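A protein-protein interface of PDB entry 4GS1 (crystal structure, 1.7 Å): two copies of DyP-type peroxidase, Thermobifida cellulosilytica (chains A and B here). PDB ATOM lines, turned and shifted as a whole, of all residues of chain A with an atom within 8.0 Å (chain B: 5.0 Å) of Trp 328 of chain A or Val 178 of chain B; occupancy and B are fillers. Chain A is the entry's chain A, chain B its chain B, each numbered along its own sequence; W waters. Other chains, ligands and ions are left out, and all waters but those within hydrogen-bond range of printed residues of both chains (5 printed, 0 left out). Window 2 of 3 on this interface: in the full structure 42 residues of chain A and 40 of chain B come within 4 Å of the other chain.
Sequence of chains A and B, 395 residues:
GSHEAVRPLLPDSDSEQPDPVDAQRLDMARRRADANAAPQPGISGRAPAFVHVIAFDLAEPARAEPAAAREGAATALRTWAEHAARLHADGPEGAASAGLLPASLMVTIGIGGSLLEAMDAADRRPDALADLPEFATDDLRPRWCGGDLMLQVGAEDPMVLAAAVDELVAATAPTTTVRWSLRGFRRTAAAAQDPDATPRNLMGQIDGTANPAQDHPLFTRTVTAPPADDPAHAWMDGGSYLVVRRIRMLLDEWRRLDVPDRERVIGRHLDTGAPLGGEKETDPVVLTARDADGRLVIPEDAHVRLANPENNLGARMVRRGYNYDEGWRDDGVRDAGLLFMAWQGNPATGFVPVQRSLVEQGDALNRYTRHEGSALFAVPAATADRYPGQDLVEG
The guanidinium group (NH2) of Arg 334 of chain A is in salt-bridge range of the side-chain carboxylate (OD1) of Asp 166 of chain B.
The side-chain carboxylate (OD1) of Asp 325 of chain A lies within hydrogen-bond range of the backbone NH (N) of Gly 327 of chain A.
The side-chain carboxylate (OD1) of Asp 325 of chain A is in salt-bridge range of the guanidinium group (NH1) of Arg 334 of chain A.
The guanidinium group of Arg 334 of chain A sits at hydrogen-bond distance from the backbone carbonyl oxygen of Gly 327 of chain A.
The backbone NH of Asp 335 of chain A lies within hydrogen-bond range of the backbone carbonyl oxygen of Gly 327 of chain A (2.8 Å).
NE2 of His 52 of chain B is in hydrogen-bond range of OG of Ser 181 of chain B (3.3 Å).
Water W5 bridges OD2 of Asp 325 of chain A (2.7 Å) and ND1 of His 52 of chain B (2.9 Å).
Water W4 bridges the side-chain hydroxyl of Ser 181 of chain B and the backbone NH of Trp 328 of chain A.
Water W3 lies within hydrogen-bond range of the side-chain carboxylate of Asp 166 of chain B, the guanidinium group of Arg 255 of chain A and the guanidinium group of Arg 334 of chain A.
Water W1 bridges the backbone carbonyl oxygen of Asp 166 of chain B (3.0 Å) and the guanidinium group of Arg 255 of chain A (3.5 Å).
Water W2 lies within hydrogen-bond range of the backbone carbonyl oxygen of Trp 328 of chain A and the backbone carbonyl oxygen of Arg 179 of chain B.
No position is printed for both chains.
Of the printed residues of chain B, Trp 328 of chain A touches His 52, Val 165, Val 169, Val 178 and Ser 181.
Of chain A, only Trp 328 (3.9 Å) comes within 4 Å of Val 178 of chain B.
Of the printed residues of chain A, Val 169 of chain B touches Trp 328.
Of the printed residues of chain B, Arg 334 of chain A touches Asp 166.
Of the printed residues of chain A, Asp 166 of chain B touches Arg 334 (2.8 Å).
Printed residues of chain A within 4 Å of His 52 of chain B: Asp 325 (3.8 Å) and Trp 328 (3.9 Å).
The nearest residue of chain B that does not touch Trp 328 of chain A is Ile 54 of chain B (4.5 Å).
The nearest residue of chain A that does not touch Val 178 of chain B is Gly 332 of chain A (6.2 Å).
The nearest printed residue of chain A that does not touch His 52 of chain B is Gly 327 of chain A (4.8 Å).
Printed residues of chain A that touch a printed residue of chain B: Asp 325, Gly 327, Trp 328 and Arg 334.
Of the 13 printed residues of chain B, 6 touch a printed residue of chain A.
Along chain B the printed residues that touch a printed residue of chain A span positions 52 to 181.
Among the printed residues, 8 pairs touch across the chains.
Among the printed residues, pairs that only touch across the chains: Asp 325 of chain A with His 52 of chain B (3.8 Å), Gly 327 of chain A with Ser 181 of chain B (3.9 Å), Trp 328 of chain A with His 52 of chain B (3.9 Å), Trp 328 of chain A with Val 165 of chain B (3.9 Å), Trp 328 of chain A with Val 169 of chain B (3.9 Å), Trp 328 of chain A with Val 178 of chain B (3.9 Å) and Trp 328 of chain A with Ser 181 of chain B (3.5 Å).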
ATOM      1  N   ARG A 255      26.938  28.957  25.804  1.00  0.00           N
ATOM      2  CA  ARG A 255      26.341  29.294  27.101  1.00  0.00           C
ATOM      3  C   ARG A 255      27.263  30.097  28.023  1.00  0.00           C
ATOM      4  O   ARG A 255      26.795  30.749  28.959  1.00  0.00           O
ATOM      5  CB  ARG A 255      25.843  28.034  27.820  1.00  0.00           C
ATOM      6  CG  ARG A 255      24.530  27.492  27.268  1.00  0.00           C
ATOM      7  CD  ARG A 255      23.963  26.387  28.164  1.00  0.00           C
ATOM      8  NE  ARG A 255      24.810  25.197  28.173  1.00  0.00           N
ATOM      9  CZ  ARG A 255      24.700  24.194  27.304  1.00  0.00           C
ATOM     10  NH1 ARG A 255      23.784  24.242  26.340  1.00  0.00           N
ATOM     11  NH2 ARG A 255      25.510  23.149  27.390  1.00  0.00           N
ATOM     12  N   ASP A 325      18.083  18.074  16.566  1.00  0.00           N
ATOM     13  CA  ASP A 325      18.527  17.592  17.869  1.00  0.00           C
ATOM     14  C   ASP A 325      18.753  16.091  17.771  1.00  0.00           C
ATOM     15  O   ASP A 325      17.803  15.305  17.642  1.00  0.00           O
ATOM     16  CB  ASP A 325      17.483  17.934  18.948  1.00  0.00           C
ATOM     17  CG  ASP A 325      17.932  17.556  20.354  1.00  0.00           C
ATOM     18  OD1 ASP A 325      18.820  16.681  20.500  1.00  0.00           O
ATOM     19  OD2 ASP A 325      17.402  18.129  21.338  1.00  0.00           O
ATOM     20  N   GLU A 326      20.022  15.700  17.819  1.00  0.00           N
ATOM     21  CA  GLU A 326      20.393  14.296  17.757  1.00  0.00           C
ATOM     22  C   GLU A 326      21.105  13.862  19.027  1.00  0.00           C
ATOM     23  O   GLU A 326      21.950  12.958  19.008  1.00  0.00           O
ATOM     24  CB  GLU A 326      21.240  14.021  16.505  1.00  0.00           C
ATOM     25  CG  GLU A 326      20.425  14.116  15.199  1.00  0.00           C
ATOM     26  CD  GLU A 326      19.256  13.141  15.178  1.00  0.00           C
ATOM     27  OE1 GLU A 326      19.443  12.022  15.664  1.00  0.00           O
ATOM     28  OE2 GLU A 326      18.143  13.486  14.711  1.00  0.00           O
ATOM     29  N   GLY A 327      20.738  14.498  20.139  1.00  0.00           N
ATOM     30  CA  GLY A 327      21.212  14.070  21.443  1.00  0.00           C
ATOM     31  C   GLY A 327      22.693  14.309  21.669  1.00  0.00           C
ATOM     32  O   GLY A 327      23.180  15.411  21.416  1.00  0.00           O
ATOM     33  N   TRP A 328      23.386  13.284  22.177  1.00  0.00           N
ATOM     34  CA  TRP A 328      24.811  13.370  22.523  1.00  0.00           C
ATOM     35  C   TRP A 328      25.578  12.243  21.835  1.00  0.00           C
ATOM     36  O   TRP A 328      25.126  11.096  21.816  1.00  0.00           O
ATOM     37  CB  TRP A 328      25.002  13.290  24.054  1.00  0.00           C
ATOM     38  CG  TRP A 328      24.521  14.533  24.757  1.00  0.00           C
ATOM     39  CD1 TRP A 328      25.285  15.579  25.182  1.00  0.00           C
ATOM     40  CD2 TRP A 328      23.156  14.876  25.077  1.00  0.00           C
ATOM     41  NE1 TRP A 328      24.486  16.555  25.753  1.00  0.00           N
ATOM     42  CE2 TRP A 328      23.177  16.143  25.695  1.00  0.00           C
ATOM     43  CE3 TRP A 328      21.924  14.226  24.908  1.00  0.00           C
ATOM     44  CZ2 TRP A 328      22.013  16.785  26.138  1.00  0.00           C
ATOM     45  CZ3 TRP A 328      20.764  14.871  25.341  1.00  0.00           C
ATOM     46  CH2 TRP A 328      20.822  16.135  25.951  1.00  0.00           C
ATOM     47  N   ARG A 329      26.721  12.580  21.251  1.00  0.00           N
ATOM     48  CA  ARG A 329      27.592  11.591  20.614  1.00  0.00           C
ATOM     49  C   ARG A 329      28.273  10.740  21.668  1.00  0.00           C
ATOM     50  O   ARG A 329      28.227  11.065  22.854  1.00  0.00           O
ATOM     51  CB  ARG A 329      28.674  12.295  19.779  1.00  0.00           C
ATOM     52  CG  ARG A 329      28.124  13.279  18.755  1.00  0.00           C
ATOM     53  CD  ARG A 329      29.163  13.658  17.701  1.00  0.00           C
ATOM     54  NE  ARG A 329      30.424  14.150  18.259  1.00  0.00           N
ATOM     55  CZ  ARG A 329      31.175  15.096  17.698  1.00  0.00           C
ATOM     56  NH1 ARG A 329      32.323  15.465  18.257  1.00  0.00           N
ATOM     57  NH2 ARG A 329      30.776  15.676  16.574  1.00  0.00           N
ATOM     58  N   ASP A 330      28.917   9.654  21.240  1.00  0.00           N
ATOM     59  CA  ASP A 330      29.626   8.791  22.177  1.00  0.00           C
ATOM     60  C   ASP A 330      30.740   9.535  22.896  1.00  0.00           C
ATOM     61  O   ASP A 330      31.079   9.200  24.039  1.00  0.00           O
ATOM     62  CB  ASP A 330      30.203   7.566  21.455  1.00  0.00           C
ATOM     63  CG  ASP A 330      29.142   6.562  21.063  1.00  0.00           C
ATOM     64  OD1 ASP A 330      28.008   6.655  21.579  1.00  0.00           O
ATOM     65  OD2 ASP A 330      29.452   5.667  20.245  1.00  0.00           O
ATOM     66  N   ASP A 331      31.305  10.541  22.235  1.00  0.00           N
ATOM     67  CA  ASP A 331      32.398  11.312  22.835  1.00  0.00           C
ATOM     68  C   ASP A 331      31.892  12.409  23.769  1.00  0.00           C
ATOM     69  O   ASP A 331      32.676  13.175  24.327  1.00  0.00           O
ATOM     70  CB  ASP A 331      33.357  11.879  21.767  1.00  0.00           C
ATOM     71  CG  ASP A 331      32.749  13.011  20.945  1.00  0.00           C
ATOM     72  OD1 ASP A 331      31.514  13.226  20.982  1.00  0.00           O
ATOM     73  OD2 ASP A 331      33.524  13.708  20.242  1.00  0.00           O
ATOM     74  N   GLY A 332      30.574  12.477  23.947  1.00  0.00           N
ATOM     75  CA  GLY A 332      29.982  13.412  24.891  1.00  0.00           C
ATOM     76  C   GLY A 332      29.499  14.708  24.285  1.00  0.00           C
ATOM     77  O   GLY A 332      28.794  15.486  24.947  1.00  0.00           O
ATOM     78  N   VAL A 333      29.874  14.963  23.035  1.00  0.00           N
ATOM     79  CA  VAL A 333      29.537  16.228  22.400  1.00  0.00           C
ATOM     80  C   VAL A 333      28.046  16.316  22.068  1.00  0.00           C
ATOM     81  O   VAL A 333      27.449  15.347  21.592  1.00  0.00           O
ATOM     82  CB  VAL A 333      30.389  16.430  21.131  1.00  0.00           C
ATOM     83  CG1 VAL A 333      29.865  17.597  20.305  1.00  0.00           C
ATOM     84  CG2 VAL A 333      31.846  16.667  21.524  1.00  0.00           C
ATOM     85  N   ARG A 334      27.446  17.482  22.312  1.00  0.00           N
ATOM     86  CA  ARG A 334      26.037  17.697  21.979  1.00  0.00           C
ATOM     87  C   ARG A 334      25.874  17.757  20.463  1.00  0.00           C
ATOM     88  O   ARG A 334      26.484  18.601  19.803  1.00  0.00           O
ATOM     89  CB  ARG A 334      25.561  19.016  22.601  1.00  0.00           C
ATOM     90  CG  ARG A 334      24.076  19.314  22.401  1.00  0.00           C
ATOM     91  CD  ARG A 334      23.219  18.580  23.426  1.00  0.00           C
ATOM     92  NE  ARG A 334      21.853  19.115  23.458  1.00  0.00           N
ATOM     93  CZ  ARG A 334      20.836  18.592  22.786  1.00  0.00           C
ATOM     94  NH1 ARG A 334      21.019  17.512  22.022  1.00  0.00           N
ATOM     95  NH2 ARG A 334      19.633  19.147  22.870  1.00  0.00           N
ATOM     96  N   ASP A 335      25.063  16.859  19.907  1.00  0.00           N
ATOM     97  CA  ASP A 335      24.877  16.807  18.458  1.00  0.00           C
ATOM     98  C   ASP A 335      23.559  17.474  18.125  1.00  0.00           C
ATOM     99  O   ASP A 335      22.528  16.808  17.972  1.00  0.00           O
ATOM    100  CB  ASP A 335      24.864  15.366  17.951  1.00  0.00           C
ATOM    101  CG  ASP A 335      25.138  15.278  16.456  1.00  0.00           C
ATOM    102  OD1 ASP A 335      24.927  16.286  15.751  1.00  0.00           O
ATOM    103  OD2 ASP A 335      25.564  14.209  15.985  1.00  0.00           O
ATOM    104  N   ALA A 336      23.606  18.797  18.036  1.00  0.00           N
ATOM    105  CA  ALA A 336      22.431  19.614  17.770  1.00  0.00           C
ATOM    106  C   ALA A 336      22.895  20.839  17.019  1.00  0.00           C
ATOM    107  O   ALA A 336      24.070  21.219  17.098  1.00  0.00           O
ATOM    108  CB  ALA A 336      21.759  20.018  19.096  1.00  0.00           C
ATOM    109  N   HIS B  52      11.616  13.646  25.476  1.00  0.00           N
ATOM    110  CA  HIS B  52      13.053  13.389  25.399  1.00  0.00           C
ATOM    111  C   HIS B  52      13.393  12.662  26.687  1.00  0.00           C
ATOM    112  O   HIS B  52      13.229  13.210  27.782  1.00  0.00           O
ATOM    113  CB  HIS B  52      13.846  14.704  25.263  1.00  0.00           C
ATOM    114  CG  HIS B  52      15.227  14.533  24.701  1.00  0.00           C
ATOM    115  ND1 HIS B  52      15.892  15.549  24.032  1.00  0.00           N
ATOM    116  CD2 HIS B  52      16.079  13.478  24.716  1.00  0.00           C
ATOM    117  CE1 HIS B  52      17.082  15.120  23.655  1.00  0.00           C
ATOM    118  NE2 HIS B  52      17.226  13.864  24.055  1.00  0.00           N
ATOM    119  N   ILE B  54      16.250  11.010  28.956  1.00  0.00           N
ATOM    120  CA  ILE B  54      17.700  11.115  29.107  1.00  0.00           C
ATOM    121  C   ILE B  54      18.164  10.327  30.318  1.00  0.00           C
ATOM    122  O   ILE B  54      17.686  10.551  31.433  1.00  0.00           O
ATOM    123  CB  ILE B  54      18.145  12.588  29.285  1.00  0.00           C
ATOM    124  CG1 ILE B  54      17.541  13.460  28.181  1.00  0.00           C
ATOM    125  CG2 ILE B  54      19.680  12.695  29.251  1.00  0.00           C
ATOM    126  CD1 ILE B  54      17.152  14.842  28.638  1.00  0.00           C
ATOM    127  N   ALA B  55      19.100   9.406  30.102  1.00  0.00           N
ATOM    128  CA  ALA B  55      19.694   8.658  31.209  1.00  0.00           C
ATOM    129  C   ALA B  55      21.060   9.252  31.519  1.00  0.00           C
ATOM    130  O   ALA B  55      21.820   9.584  30.606  1.00  0.00           O
ATOM    131  CB  ALA B  55      19.825   7.169  30.846  1.00  0.00           C
ATOM    132  N   PHE B  56      21.360   9.420  32.805  1.00  0.00           N
ATOM    133  CA  PHE B  56      22.635  10.019  33.228  1.00  0.00           C
ATOM    134  C   PHE B  56      23.398   9.081  34.144  1.00  0.00           C
ATOM    135  O   PHE B  56      22.792   8.293  34.869  1.00  0.00           O
ATOM    136  CB  PHE B  56      22.390  11.277  34.066  1.00  0.00           C
ATOM    137  CG  PHE B  56      21.623  12.377  33.361  1.00  0.00           C
ATOM    138  CD1 PHE B  56      22.294  13.476  32.829  1.00  0.00           C
ATOM    139  CD2 PHE B  56      20.233  12.348  33.290  1.00  0.00           C
ATOM    140  CE1 PHE B  56      21.588  14.511  32.222  1.00  0.00           C
ATOM    141  CE2 PHE B  56      19.525  13.376  32.678  1.00  0.00           C
ATOM    142  CZ  PHE B  56      20.197  14.452  32.142  1.00  0.00           C
ATOM    143  N   VAL B 165      15.250  20.814  27.895  1.00  0.00           N
ATOM    144  CA  VAL B 165      16.266  19.777  27.981  1.00  0.00           C
ATOM    145  C   VAL B 165      17.666  20.364  28.157  1.00  0.00           C
ATOM    146  O   VAL B 165      18.426  19.928  29.028  1.00  0.00           O
ATOM    147  CB  VAL B 165      16.225  18.880  26.743  1.00  0.00           C
ATOM    148  CG1 VAL B 165      17.501  18.031  26.648  1.00  0.00           C
ATOM    149  CG2 VAL B 165      14.995  17.983  26.802  1.00  0.00           C
ATOM    150  N   ASP B 166      18.002  21.359  27.347  1.00  0.00           N
ATOM    151  CA  ASP B 166      19.345  21.942  27.416  1.00  0.00           C
ATOM    152  C   ASP B 166      19.569  22.597  28.775  1.00  0.00           C
ATOM    153  O   ASP B 166      20.656  22.500  29.362  1.00  0.00           O
ATOM    154  CB  ASP B 166      19.572  22.930  26.261  1.00  0.00           C
ATOM    155  CG  ASP B 166      19.683  22.232  24.900  1.00  0.00           C
ATOM    156  OD1 ASP B 166      20.025  21.034  24.875  1.00  0.00           O
ATOM    157  OD2 ASP B 166      19.429  22.884  23.858  1.00  0.00           O
ATOM    158  N   VAL B 169      20.035  19.658  31.524  1.00  0.00           N
ATOM    159  CA  VAL B 169      21.293  18.925  31.399  1.00  0.00           C
ATOM    160  C   VAL B 169      22.472  19.803  31.813  1.00  0.00           C
ATOM    161  O   VAL B 169      23.367  19.362  32.533  1.00  0.00           O
ATOM    162  CB  VAL B 169      21.490  18.407  29.965  1.00  0.00           C
ATOM    163  CG1 VAL B 169      22.882  17.802  29.801  1.00  0.00           C
ATOM    164  CG2 VAL B 169      20.426  17.369  29.647  1.00  0.00           C
ATOM    165  N   THR B 176      26.893  15.280  36.675  1.00  0.00           N
ATOM    166  CA  THR B 176      26.232  14.251  35.862  1.00  0.00           C
ATOM    167  C   THR B 176      26.783  14.245  34.438  1.00  0.00           C
ATOM    168  O   THR B 176      27.248  15.274  33.944  1.00  0.00           O
ATOM    169  CB  THR B 176      24.706  14.465  35.774  1.00  0.00           C
ATOM    170  OG1 THR B 176      24.431  15.780  35.276  1.00  0.00           O
ATOM    171  CG2 THR B 176      24.035  14.291  37.128  1.00  0.00           C
ATOM    172  N   THR B 177      26.720  13.083  33.787  1.00  0.00           N
ATOM    173  CA  THR B 177      27.101  12.934  32.382  1.00  0.00           C
ATOM    174  C   THR B 177      25.993  12.161  31.672  1.00  0.00           C
ATOM    175  O   THR B 177      25.482  11.184  32.217  1.00  0.00           O
ATOM    176  CB  THR B 177      28.403  12.128  32.236  1.00  0.00           C
ATOM    177  OG1 THR B 177      29.431  12.712  33.049  1.00  0.00           O
ATOM    178  CG2 THR B 177      28.853  12.126  30.786  1.00  0.00           C
ATOM    179  N   VAL B 178      25.613  12.589  30.472  1.00  0.00           N
ATOM    180  CA  VAL B 178      24.620  11.837  29.703  1.00  0.00           C
ATOM    181  C   VAL B 178      25.148  10.460  29.305  1.00  0.00           C
ATOM    182  O   VAL B 178      26.242  10.341  28.736  1.00  0.00           O
ATOM    183  CB  VAL B 178      24.161  12.602  28.444  1.00  0.00           C
ATOM    184  CG1 VAL B 178      23.266  11.724  27.590  1.00  0.00           C
ATOM    185  CG2 VAL B 178      23.398  13.866  28.831  1.00  0.00           C
ATOM    186  N   ARG B 179      24.375   9.420  29.614  1.00  0.00           N
ATOM    187  CA  ARG B 179      24.719   8.055  29.218  1.00  0.00           C
ATOM    188  C   ARG B 179      24.092   7.691  27.871  1.00  0.00           C
ATOM    189  O   ARG B 179      24.785   7.239  26.951  1.00  0.00           O
ATOM    190  CB  ARG B 179      24.277   7.053  30.295  1.00  0.00           C
ATOM    191  CG  ARG B 179      24.689   5.614  30.025  1.00  0.00           C
ATOM    192  CD  ARG B 179      24.231   4.679  31.163  1.00  0.00           C
ATOM    193  NE  ARG B 179      24.591   3.287  30.880  1.00  0.00           N
ATOM    194  CZ  ARG B 179      25.750   2.735  31.228  1.00  0.00           C
ATOM    195  NH1 ARG B 179      26.666   3.444  31.888  1.00  0.00           N
ATOM    196  NH2 ARG B 179      25.999   1.473  30.917  1.00  0.00           N
ATOM    197  N   TRP B 180      22.784   7.892  27.762  1.00  0.00           N
ATOM    198  CA  TRP B 180      22.077   7.727  26.496  1.00  0.00           C
ATOM    199  C   TRP B 180      20.847   8.629  26.520  1.00  0.00           C
ATOM    200  O   TRP B 180      20.415   9.080  27.577  1.00  0.00           O
ATOM    201  CB  TRP B 180      21.701   6.251  26.210  1.00  0.00           C
ATOM    202  CG  TRP B 180      20.795   5.595  27.231  1.00  0.00           C
ATOM    203  CD1 TRP B 180      21.180   4.789  28.283  1.00  0.00           C
ATOM    204  CD2 TRP B 180      19.368   5.681  27.303  1.00  0.00           C
ATOM    205  NE1 TRP B 180      20.072   4.379  28.994  1.00  0.00           N
ATOM    206  CE2 TRP B 180      18.950   4.915  28.413  1.00  0.00           C
ATOM    207  CE3 TRP B 180      18.399   6.338  26.530  1.00  0.00           C
ATOM    208  CZ2 TRP B 180      17.608   4.785  28.772  1.00  0.00           C
ATOM    209  CZ3 TRP B 180      17.057   6.209  26.890  1.00  0.00           C
ATOM    210  CH2 TRP B 180      16.677   5.443  28.005  1.00  0.00           C
ATOM    211  N   SER B 181      20.296   8.922  25.352  1.00  0.00           N
ATOM    212  CA  SER B 181      19.038   9.655  25.311  1.00  0.00           C
ATOM    213  C   SER B 181      18.274   9.275  24.064  1.00  0.00           C
ATOM    214  O   SER B 181      18.849   8.756  23.106  1.00  0.00           O
ATOM    215  CB  SER B 181      19.272  11.170  25.356  1.00  0.00           C
ATOM    216  OG  SER B 181      19.635  11.662  24.071  1.00  0.00           O
HETATM  217  O   HOH W   1      22.766  21.081  27.813  1.00  0.00           O
HETATM  218  O   HOH W   2      24.536   9.493  24.459  1.00  0.00           O
HETATM  219  O   HOH W   3      22.820  21.755  24.914  1.00  0.00           O
HETATM  220  O   HOH W   4      21.935  10.810  22.883  1.00  0.00           O
HETATM  221  O   HOH W   5      14.992  17.819  22.533  1.00  0.00           O
